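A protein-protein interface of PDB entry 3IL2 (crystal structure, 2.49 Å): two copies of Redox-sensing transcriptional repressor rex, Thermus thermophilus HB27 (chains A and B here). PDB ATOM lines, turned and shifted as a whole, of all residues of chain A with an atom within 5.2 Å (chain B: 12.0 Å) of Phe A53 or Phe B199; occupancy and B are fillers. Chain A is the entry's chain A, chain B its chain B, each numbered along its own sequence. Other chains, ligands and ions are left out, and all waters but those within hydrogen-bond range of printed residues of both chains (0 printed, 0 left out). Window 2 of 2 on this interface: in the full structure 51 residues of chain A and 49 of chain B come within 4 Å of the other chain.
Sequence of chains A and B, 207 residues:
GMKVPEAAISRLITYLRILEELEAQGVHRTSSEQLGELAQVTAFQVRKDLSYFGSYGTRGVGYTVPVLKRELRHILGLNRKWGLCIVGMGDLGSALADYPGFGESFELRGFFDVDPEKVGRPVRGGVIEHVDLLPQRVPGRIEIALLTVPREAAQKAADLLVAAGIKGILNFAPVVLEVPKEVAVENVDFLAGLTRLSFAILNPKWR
Of the 18 printed residues of chain B, 4 touch a printed residue of chain A. Hydrophobic or aromatic side chains of chain B within 4 Å of the printed part of chain A: Phe B199 and Trp B206. Of the 13 printed residues of chain A, 5 touch a printed residue of chain B. Among the printed residues, 8 pairs touch across the chains. Among the printed residues, no Asp or Glu carboxylate lies within 4 Å of a Lys or Arg side-chain nitrogen of the other chain.
The indole nitrogen (NE1) of Trp B206 lies within hydrogen-bond range of the backbone carbonyl oxygen (O) of Val A4 (2.9 Å). O of Leu A76 is in hydrogen-bond range of OG of Ser B198 (2.5 Å).
Val A4 touches just one residue of chain B: Trp B206 (2.9 Å). No residue of chain B comes within 4 Å of Ser A51. Of chain B, only Phe B199 (3.9 Å) comes within 4 Å of Phe A53. No residue of chain B comes within 4 Å of Ser A55. Ile A75 touches just one residue of chain B: Phe B199. Ala B192 touches none of the printed residues of chain A. Of the printed residues of chain A, Thr B195 touches Leu A76 (3.7 Å). Of the printed residues of chain A, Ser B198 touches Leu A76 (2.5 Å). Of chain A, only Ile A9, Phe A53, Ile A75 and Leu A76 come within 4 Å of Phe B199. Of the printed residues of chain A, Trp B206 touches Val A4 and Ile A9. The nearest residue of chain B that does not touch Phe A53 is Asn B203 (6.0 Å). The nearest residue of chain A that does not touch Phe B199 is Val A4 (5.1 Å). The nearest printed residue of chain A that does not touch Thr B195 is Ile A9 (5.8 Å).
No position is printed for both chains. Of the 8 pairs that touch across the chains among the printed residues, none has its exchanged pair printed and touching as well.
The side-chain hydroxyl of Tyr A56 sits at hydrogen-bond distance from the backbone carbonyl oxygen of Phe A53 (2.8 Å). The side-chain hydroxyl (OG1) of Thr B195 lies within hydrogen-bond range of the backbone carbonyl oxygen (O) of Leu B191 (3.0 Å). The backbone carbonyl oxygen (O) of Phe B199 sits close to the side-chain amide oxygen (OD1) of Asn B203, at 3.0 Å.
Among the printed residues, merely in contact across the chains: Ile A9 with Phe B199, Ile A75 with Phe B199, Leu A76 with Phe B199, Leu A76 with Thr B195, Ile A9 with Trp B206 and Phe A53 with Phe B199.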
ATOM      1  N   VAL A   4      -2.511  13.243  29.655  1.00  0.00           N
ATOM      2  CA  VAL A   4      -2.562  11.862  29.222  1.00  0.00           C
ATOM      3  C   VAL A   4      -2.449  10.839  30.314  1.00  0.00           C
ATOM      4  O   VAL A   4      -1.485  10.843  31.063  1.00  0.00           O
ATOM      5  CB  VAL A   4      -1.420  11.578  28.300  1.00  0.00           C
ATOM      6  CG1 VAL A   4      -1.718  10.399  27.470  1.00  0.00           C
ATOM      7  CG2 VAL A   4      -1.163  12.763  27.464  1.00  0.00           C
ATOM      8  N   ILE A   9      -0.389   5.267  27.419  1.00  0.00           N
ATOM      9  CA  ILE A   9       0.879   5.118  26.760  1.00  0.00           C
ATOM     10  C   ILE A   9       1.280   3.674  26.611  1.00  0.00           C
ATOM     11  O   ILE A   9       2.080   3.342  25.750  1.00  0.00           O
ATOM     12  CB  ILE A   9       1.963   5.845  27.479  1.00  0.00           C
ATOM     13  CG1 ILE A   9       2.060   7.253  26.934  1.00  0.00           C
ATOM     14  CG2 ILE A   9       3.260   5.244  27.177  1.00  0.00           C
ATOM     15  CD1 ILE A   9       1.516   8.215  27.828  1.00  0.00           C
ATOM     16  N   LEU A  12      -0.550   2.729  23.449  1.00  0.00           N
ATOM     17  CA  LEU A  12       0.013   3.245  22.208  1.00  0.00           C
ATOM     18  C   LEU A  12       1.141   2.332  21.771  1.00  0.00           C
ATOM     19  O   LEU A  12       1.303   2.038  20.588  1.00  0.00           O
ATOM     20  CB  LEU A  12       0.555   4.667  22.392  1.00  0.00           C
ATOM     21  CG  LEU A  12      -0.447   5.791  22.617  1.00  0.00           C
ATOM     22  CD1 LEU A  12       0.300   7.104  22.566  1.00  0.00           C
ATOM     23  CD2 LEU A  12      -1.545   5.756  21.539  1.00  0.00           C
ATOM     24  N   ASP A  49      -7.211   7.314  22.927  1.00  0.00           N
ATOM     25  CA  ASP A  49      -5.778   7.267  23.165  1.00  0.00           C
ATOM     26  C   ASP A  49      -5.071   8.091  22.112  1.00  0.00           C
ATOM     27  O   ASP A  49      -4.003   8.635  22.359  1.00  0.00           O
ATOM     28  CB  ASP A  49      -5.255   5.830  23.115  1.00  0.00           C
ATOM     29  CG  ASP A  49      -5.723   4.999  24.282  1.00  0.00           C
ATOM     30  OD1 ASP A  49      -5.803   5.534  25.410  1.00  0.00           O
ATOM     31  OD2 ASP A  49      -5.996   3.800  24.072  1.00  0.00           O
ATOM     32  N   LEU A  50      -5.671   8.183  20.931  1.00  0.00           N
ATOM     33  CA  LEU A  50      -5.076   8.943  19.842  1.00  0.00           C
ATOM     34  C   LEU A  50      -5.384  10.430  19.907  1.00  0.00           C
ATOM     35  O   LEU A  50      -4.564  11.253  19.512  1.00  0.00           O
ATOM     36  CB  LEU A  50      -5.541   8.396  18.494  1.00  0.00           C
ATOM     37  CG  LEU A  50      -5.052   7.004  18.113  1.00  0.00           C
ATOM     38  CD1 LEU A  50      -5.570   6.673  16.729  1.00  0.00           C
ATOM     39  CD2 LEU A  50      -3.528   6.949  18.138  1.00  0.00           C
ATOM     40  N   SER A  51      -6.559  10.775  20.413  1.00  0.00           N
ATOM     41  CA  SER A  51      -6.953  12.179  20.490  1.00  0.00           C
ATOM     42  C   SER A  51      -6.052  13.010  21.398  1.00  0.00           C
ATOM     43  O   SER A  51      -5.910  14.213  21.194  1.00  0.00           O
ATOM     44  CB  SER A  51      -8.408  12.305  20.958  1.00  0.00           C
ATOM     45  OG  SER A  51      -8.564  11.858  22.292  1.00  0.00           O
ATOM     46  N   TYR A  52      -5.435  12.381  22.393  1.00  0.00           N
ATOM     47  CA  TYR A  52      -4.561  13.126  23.296  1.00  0.00           C
ATOM     48  C   TYR A  52      -3.396  13.745  22.530  1.00  0.00           C
ATOM     49  O   TYR A  52      -2.767  14.697  23.001  1.00  0.00           O
ATOM     50  CB  TYR A  52      -3.975  12.226  24.388  1.00  0.00           C
ATOM     51  CG  TYR A  52      -4.976  11.499  25.250  1.00  0.00           C
ATOM     52  CD1 TYR A  52      -5.071  10.109  25.204  1.00  0.00           C
ATOM     53  CD2 TYR A  52      -5.807  12.189  26.138  1.00  0.00           C
ATOM     54  CE1 TYR A  52      -5.962   9.423  26.020  1.00  0.00           C
ATOM     55  CE2 TYR A  52      -6.705  11.505  26.965  1.00  0.00           C
ATOM     56  CZ  TYR A  52      -6.771  10.123  26.896  1.00  0.00           C
ATOM     57  OH  TYR A  52      -7.623   9.428  27.707  1.00  0.00           O
ATOM     58  N   PHE A  53      -3.101  13.209  21.350  1.00  0.00           N
ATOM     59  CA  PHE A  53      -1.977  13.729  20.595  1.00  0.00           C
ATOM     60  C   PHE A  53      -2.295  14.349  19.249  1.00  0.00           C
ATOM     61  O   PHE A  53      -1.503  15.129  18.731  1.00  0.00           O
ATOM     62  CB  PHE A  53      -0.921  12.635  20.421  1.00  0.00           C
ATOM     63  CG  PHE A  53      -0.406  12.087  21.722  1.00  0.00           C
ATOM     64  CD1 PHE A  53      -1.078  11.063  22.373  1.00  0.00           C
ATOM     65  CD2 PHE A  53       0.741  12.616  22.310  1.00  0.00           C
ATOM     66  CE1 PHE A  53      -0.618  10.569  23.586  1.00  0.00           C
ATOM     67  CE2 PHE A  53       1.205  12.132  23.521  1.00  0.00           C
ATOM     68  CZ  PHE A  53       0.529  11.106  24.160  1.00  0.00           C
ATOM     69  N   GLY A  54      -3.439  14.012  18.669  1.00  0.00           N
ATOM     70  CA  GLY A  54      -3.767  14.594  17.381  1.00  0.00           C
ATOM     71  C   GLY A  54      -4.792  13.843  16.567  1.00  0.00           C
ATOM     72  O   GLY A  54      -5.320  12.815  16.990  1.00  0.00           O
ATOM     73  N   SER A  55      -5.072  14.370  15.381  1.00  0.00           N
ATOM     74  CA  SER A  55      -6.051  13.783  14.461  1.00  0.00           C
ATOM     75  C   SER A  55      -5.282  13.235  13.279  1.00  0.00           C
ATOM     76  O   SER A  55      -5.051  13.914  12.276  1.00  0.00           O
ATOM     77  CB  SER A  55      -7.031  14.853  14.018  1.00  0.00           C
ATOM     78  OG  SER A  55      -7.515  15.560  15.143  1.00  0.00           O
ATOM     79  N   TYR A  56      -4.899  11.978  13.418  1.00  0.00           N
ATOM     80  CA  TYR A  56      -4.098  11.330  12.399  1.00  0.00           C
ATOM     81  C   TYR A  56      -5.022  10.562  11.537  1.00  0.00           C
ATOM     82  O   TYR A  56      -4.609   9.792  10.673  1.00  0.00           O
ATOM     83  CB  TYR A  56      -3.155  10.366  13.108  1.00  0.00           C
ATOM     84  CG  TYR A  56      -2.480  11.007  14.268  1.00  0.00           C
ATOM     85  CD1 TYR A  56      -2.774  10.614  15.564  1.00  0.00           C
ATOM     86  CD2 TYR A  56      -1.557  12.027  14.067  1.00  0.00           C
ATOM     87  CE1 TYR A  56      -2.165  11.216  16.628  1.00  0.00           C
ATOM     88  CE2 TYR A  56      -0.945  12.632  15.119  1.00  0.00           C
ATOM     89  CZ  TYR A  56      -1.257  12.223  16.397  1.00  0.00           C
ATOM     90  OH  TYR A  56      -0.671  12.828  17.467  1.00  0.00           O
ATOM     91  N   ILE A  75       5.469  10.060  18.771  1.00  0.00           N
ATOM     92  CA  ILE A  75       4.893  10.382  20.065  1.00  0.00           C
ATOM     93  C   ILE A  75       5.634   9.680  21.213  1.00  0.00           C
ATOM     94  O   ILE A  75       5.814  10.263  22.279  1.00  0.00           O
ATOM     95  CB  ILE A  75       3.394   9.990  20.119  1.00  0.00           C
ATOM     96  CG1 ILE A  75       2.586  10.906  19.202  1.00  0.00           C
ATOM     97  CG2 ILE A  75       2.880  10.070  21.561  1.00  0.00           C
ATOM     98  CD1 ILE A  75       1.181  10.423  18.963  1.00  0.00           C
ATOM     99  N   LEU A  76       6.064   8.440  20.988  1.00  0.00           N
ATOM    100  CA  LEU A  76       6.766   7.672  22.015  1.00  0.00           C
ATOM    101  C   LEU A  76       8.261   7.992  22.096  1.00  0.00           C
ATOM    102  O   LEU A  76       8.969   7.480  22.973  1.00  0.00           O
ATOM    103  CB  LEU A  76       6.585   6.177  21.764  1.00  0.00           C
ATOM    104  CG  LEU A  76       5.144   5.707  21.593  1.00  0.00           C
ATOM    105  CD1 LEU A  76       5.123   4.292  21.011  1.00  0.00           C
ATOM    106  CD2 LEU A  76       4.436   5.778  22.924  1.00  0.00           C
ATOM    107  N   PHE B 190       9.798  -5.828  28.859  1.00  0.00           N
ATOM    108  CA  PHE B 190      10.881  -4.902  29.086  1.00  0.00           C
ATOM    109  C   PHE B 190      11.010  -3.850  28.002  1.00  0.00           C
ATOM    110  O   PHE B 190      11.416  -2.718  28.268  1.00  0.00           O
ATOM    111  CB  PHE B 190      12.180  -5.669  29.348  1.00  0.00           C
ATOM    112  CG  PHE B 190      13.013  -5.868  28.158  1.00  0.00           C
ATOM    113  CD1 PHE B 190      13.778  -4.828  27.657  1.00  0.00           C
ATOM    114  CD2 PHE B 190      13.066  -7.105  27.542  1.00  0.00           C
ATOM    115  CE1 PHE B 190      14.568  -5.007  26.554  1.00  0.00           C
ATOM    116  CE2 PHE B 190      13.861  -7.303  26.443  1.00  0.00           C
ATOM    117  CZ  PHE B 190      14.617  -6.248  25.944  1.00  0.00           C
ATOM    118  N   LEU B 191      10.639  -4.201  26.782  1.00  0.00           N
ATOM    119  CA  LEU B 191      10.672  -3.221  25.718  1.00  0.00           C
ATOM    120  C   LEU B 191       9.578  -2.177  25.923  1.00  0.00           C
ATOM    121  O   LEU B 191       9.753  -1.009  25.559  1.00  0.00           O
ATOM    122  CB  LEU B 191      10.453  -3.884  24.396  1.00  0.00           C
ATOM    123  CG  LEU B 191      11.717  -4.528  23.894  1.00  0.00           C
ATOM    124  CD1 LEU B 191      11.409  -5.145  22.600  1.00  0.00           C
ATOM    125  CD2 LEU B 191      12.789  -3.505  23.681  1.00  0.00           C
ATOM    126  N   ALA B 192       8.439  -2.584  26.478  1.00  0.00           N
ATOM    127  CA  ALA B 192       7.382  -1.609  26.697  1.00  0.00           C
ATOM    128  C   ALA B 192       7.903  -0.621  27.729  1.00  0.00           C
ATOM    129  O   ALA B 192       7.720   0.591  27.586  1.00  0.00           O
ATOM    130  CB  ALA B 192       6.107  -2.284  27.189  1.00  0.00           C
ATOM    131  N   GLY B 193       8.570  -1.150  28.760  1.00  0.00           N
ATOM    132  CA  GLY B 193       9.136  -0.313  29.813  1.00  0.00           C
ATOM    133  C   GLY B 193      10.161   0.672  29.267  1.00  0.00           C
ATOM    134  O   GLY B 193      10.217   1.826  29.697  1.00  0.00           O
ATOM    135  N   LEU B 194      10.991   0.217  28.338  1.00  0.00           N
ATOM    136  CA  LEU B 194      11.961   1.092  27.705  1.00  0.00           C
ATOM    137  C   LEU B 194      11.272   2.218  27.007  1.00  0.00           C
ATOM    138  O   LEU B 194      11.681   3.370  27.107  1.00  0.00           O
ATOM    139  CB  LEU B 194      12.705   0.398  26.599  1.00  0.00           C
ATOM    140  CG  LEU B 194      13.915  -0.366  27.015  1.00  0.00           C
ATOM    141  CD1 LEU B 194      14.695  -0.669  25.770  1.00  0.00           C
ATOM    142  CD2 LEU B 194      14.736   0.480  27.953  1.00  0.00           C
ATOM    143  N   THR B 195      10.266   1.854  26.224  1.00  0.00           N
ATOM    144  CA  THR B 195       9.543   2.843  25.458  1.00  0.00           C
ATOM    145  C   THR B 195       8.910   3.807  26.423  1.00  0.00           C
ATOM    146  O   THR B 195       8.950   5.013  26.215  1.00  0.00           O
ATOM    147  CB  THR B 195       8.508   2.186  24.551  1.00  0.00           C
ATOM    148  OG1 THR B 195       9.184   1.273  23.674  1.00  0.00           O
ATOM    149  CG2 THR B 195       7.799   3.224  23.711  1.00  0.00           C
ATOM    150  N   ARG B 196       8.342   3.303  27.501  1.00  0.00           N
ATOM    151  CA  ARG B 196       7.791   4.210  28.476  1.00  0.00           C
ATOM    152  C   ARG B 196       8.839   5.133  29.050  1.00  0.00           C
ATOM    153  O   ARG B 196       8.533   6.252  29.469  1.00  0.00           O
ATOM    154  CB  ARG B 196       7.188   3.456  29.615  1.00  0.00           C
ATOM    155  CG  ARG B 196       5.930   2.820  29.211  1.00  0.00           C
ATOM    156  CD  ARG B 196       5.117   2.583  30.433  1.00  0.00           C
ATOM    157  NE  ARG B 196       5.585   1.381  31.093  1.00  0.00           N
ATOM    158  CZ  ARG B 196       5.382   0.166  30.600  1.00  0.00           C
ATOM    159  NH1 ARG B 196       4.710   0.014  29.455  1.00  0.00           N
ATOM    160  NH2 ARG B 196       5.857  -0.896  31.241  1.00  0.00           N
ATOM    161  N   LEU B 197      10.078   4.676  29.125  1.00  0.00           N
ATOM    162  CA  LEU B 197      11.076   5.560  29.671  1.00  0.00           C
ATOM    163  C   LEU B 197      11.363   6.666  28.705  1.00  0.00           C
ATOM    164  O   LEU B 197      11.630   7.786  29.103  1.00  0.00           O
ATOM    165  CB  LEU B 197      12.366   4.844  29.930  1.00  0.00           C
ATOM    166  CG  LEU B 197      12.661   4.297  31.309  1.00  0.00           C
ATOM    167  CD1 LEU B 197      14.138   4.132  31.289  1.00  0.00           C
ATOM    168  CD2 LEU B 197      12.280   5.216  32.445  1.00  0.00           C
ATOM    169  N   SER B 198      11.343   6.329  27.423  1.00  0.00           N
ATOM    170  CA  SER B 198      11.586   7.312  26.381  1.00  0.00           C
ATOM    171  C   SER B 198      10.570   8.448  26.531  1.00  0.00           C
ATOM    172  O   SER B 198      10.915   9.633  26.598  1.00  0.00           O
ATOM    173  CB  SER B 198      11.431   6.650  25.014  1.00  0.00           C
ATOM    174  OG  SER B 198      11.259   7.626  24.020  1.00  0.00           O
ATOM    175  N   PHE B 199       9.307   8.059  26.605  1.00  0.00           N
ATOM    176  CA  PHE B 199       8.228   9.011  26.738  1.00  0.00           C
ATOM    177  C   PHE B 199       8.369   9.847  28.018  1.00  0.00           C
ATOM    178  O   PHE B 199       8.194  11.065  28.003  1.00  0.00           O
ATOM    179  CB  PHE B 199       6.887   8.254  26.727  1.00  0.00           C
ATOM    180  CG  PHE B 199       5.696   9.148  26.700  1.00  0.00           C
ATOM    181  CD1 PHE B 199       5.329   9.786  25.526  1.00  0.00           C
ATOM    182  CD2 PHE B 199       4.992   9.423  27.863  1.00  0.00           C
ATOM    183  CE1 PHE B 199       4.284  10.694  25.503  1.00  0.00           C
ATOM    184  CE2 PHE B 199       3.939  10.332  27.855  1.00  0.00           C
ATOM    185  CZ  PHE B 199       3.588  10.970  26.667  1.00  0.00           C
ATOM    186  N   ALA B 200       8.690   9.188  29.125  1.00  0.00           N
ATOM    187  CA  ALA B 200       8.825   9.853  30.412  1.00  0.00           C
ATOM    188  C   ALA B 200       9.898  10.919  30.378  1.00  0.00           C
ATOM    189  O   ALA B 200       9.783  11.981  30.992  1.00  0.00           O
ATOM    190  CB  ALA B 200       9.150   8.835  31.477  1.00  0.00           C
ATOM    191  N   ILE B 201      10.965  10.627  29.662  1.00  0.00           N
ATOM    192  CA  ILE B 201      12.054  11.571  29.553  1.00  0.00           C
ATOM    193  C   ILE B 201      11.644  12.788  28.759  1.00  0.00           C
ATOM    194  O   ILE B 201      11.928  13.918  29.130  1.00  0.00           O
ATOM    195  CB  ILE B 201      13.238  10.971  28.817  1.00  0.00           C
ATOM    196  CG1 ILE B 201      13.669   9.693  29.497  1.00  0.00           C
ATOM    197  CG2 ILE B 201      14.387  11.934  28.832  1.00  0.00           C
ATOM    198  CD1 ILE B 201      13.696   9.865  30.933  1.00  0.00           C
ATOM    199  N   LEU B 202      10.985  12.536  27.641  1.00  0.00           N
ATOM    200  CA  LEU B 202      10.596  13.599  26.749  1.00  0.00           C
ATOM    201  C   LEU B 202       9.523  14.464  27.313  1.00  0.00           C
ATOM    202  O   LEU B 202       9.302  15.581  26.878  1.00  0.00           O
ATOM    203  CB  LEU B 202      10.099  13.007  25.455  1.00  0.00           C
ATOM    204  CG  LEU B 202      11.046  12.853  24.271  1.00  0.00           C
ATOM    205  CD1 LEU B 202      12.481  13.061  24.643  1.00  0.00           C
ATOM    206  CD2 LEU B 202      10.858  11.482  23.716  1.00  0.00           C
ATOM    207  N   ASN B 203       8.873  13.940  28.315  1.00  0.00           N
ATOM    208  CA  ASN B 203       7.779  14.635  28.866  1.00  0.00           C
ATOM    209  C   ASN B 203       7.953  14.720  30.345  1.00  0.00           C
ATOM    210  O   ASN B 203       7.217  14.092  31.093  1.00  0.00           O
ATOM    211  CB  ASN B 203       6.528  13.873  28.484  1.00  0.00           C
ATOM    212  CG  ASN B 203       6.269  13.903  26.999  1.00  0.00           C
ATOM    213  OD1 ASN B 203       6.716  13.038  26.228  1.00  0.00           O
ATOM    214  ND2 ASN B 203       5.556  14.931  26.579  1.00  0.00           N
ATOM    215  N   PRO B 204       8.975  15.463  30.783  1.00  0.00           N
ATOM    216  CA  PRO B 204       9.319  15.624  32.197  1.00  0.00           C
ATOM    217  C   PRO B 204       8.172  16.247  33.005  1.00  0.00           C
ATOM    218  O   PRO B 204       7.869  15.792  34.107  1.00  0.00           O
ATOM    219  CB  PRO B 204      10.549  16.525  32.153  1.00  0.00           C
ATOM    220  CG  PRO B 204      10.394  17.268  30.870  1.00  0.00           C
ATOM    221  CD  PRO B 204       9.927  16.203  29.935  1.00  0.00           C
ATOM    222  N   LYS B 205       7.535  17.290  32.457  1.00  0.00           N
ATOM    223  CA  LYS B 205       6.437  17.980  33.136  1.00  0.00           C
ATOM    224  C   LYS B 205       5.382  16.958  33.518  1.00  0.00           C
ATOM    225  O   LYS B 205       4.979  16.844  34.671  1.00  0.00           O
ATOM    226  CB  LYS B 205       5.848  19.045  32.204  1.00  0.00           C
ATOM    227  CG  LYS B 205       4.980  20.072  32.906  1.00  0.00           C
ATOM    228  CD  LYS B 205       3.667  19.461  33.374  1.00  0.00           C
ATOM    229  CE  LYS B 205       2.792  20.491  34.065  1.00  0.00           C
ATOM    230  NZ  LYS B 205       3.440  21.021  35.297  1.00  0.00           N
ATOM    231  N   TRP B 206       4.945  16.217  32.523  1.00  0.00           N
ATOM    232  CA  TRP B 206       3.986  15.147  32.668  1.00  0.00           C
ATOM    233  C   TRP B 206       4.368  14.181  33.783  1.00  0.00           C
ATOM    234  O   TRP B 206       3.605  13.918  34.711  1.00  0.00           O
ATOM    235  CB  TRP B 206       4.000  14.375  31.382  1.00  0.00           C
ATOM    236  CG  TRP B 206       2.992  13.400  31.333  1.00  0.00           C
ATOM    237  CD1 TRP B 206       1.655  13.619  31.227  1.00  0.00           C
ATOM    238  CD2 TRP B 206       3.182  11.998  31.324  1.00  0.00           C
ATOM    239  NE1 TRP B 206       0.992  12.428  31.142  1.00  0.00           N
ATOM    240  CE2 TRP B 206       1.911  11.413  31.199  1.00  0.00           C
ATOM    241  CE3 TRP B 206       4.308  11.173  31.407  1.00  0.00           C
ATOM    242  CZ2 TRP B 206       1.733  10.047  31.146  1.00  0.00           C
ATOM    243  CZ3 TRP B 206       4.131   9.816  31.354  1.00  0.00           C
ATOM    244  CH2 TRP B 206       2.854   9.263  31.224  1.00  0.00           C
ATOM    245  N   ARG B 207       5.559  13.620  33.641  1.00  0.00           N
ATOM    246  CA  ARG B 207       6.093  12.661  34.591  1.00  0.00           C
ATOM    247  C   ARG B 207       5.874  13.101  36.041  1.00  0.00           C
ATOM    248  O   ARG B 207       5.353  12.288  36.835  1.00  0.00           O
ATOM    249  CB  ARG B 207       7.578  12.453  34.302  1.00  0.00           C
ATOM    250  CG  ARG B 207       8.100  11.088  34.669  1.00  0.00           C
ATOM    251  CD  ARG B 207       8.651  11.047  36.086  1.00  0.00           C
ATOM    252  NE  ARG B 207       8.957   9.671  36.489  1.00  0.00           N
ATOM    253  CZ  ARG B 207       9.458   9.311  37.670  1.00  0.00           C
ATOM    254  NH1 ARG B 207       9.691   8.027  37.917  1.00  0.00           N
ATOM    255  NH2 ARG B 207       9.731  10.224  38.597  1.00  0.00           N
ATOM    256  OXT ARG B 207       6.222  14.253  36.376  1.00  0.00           O
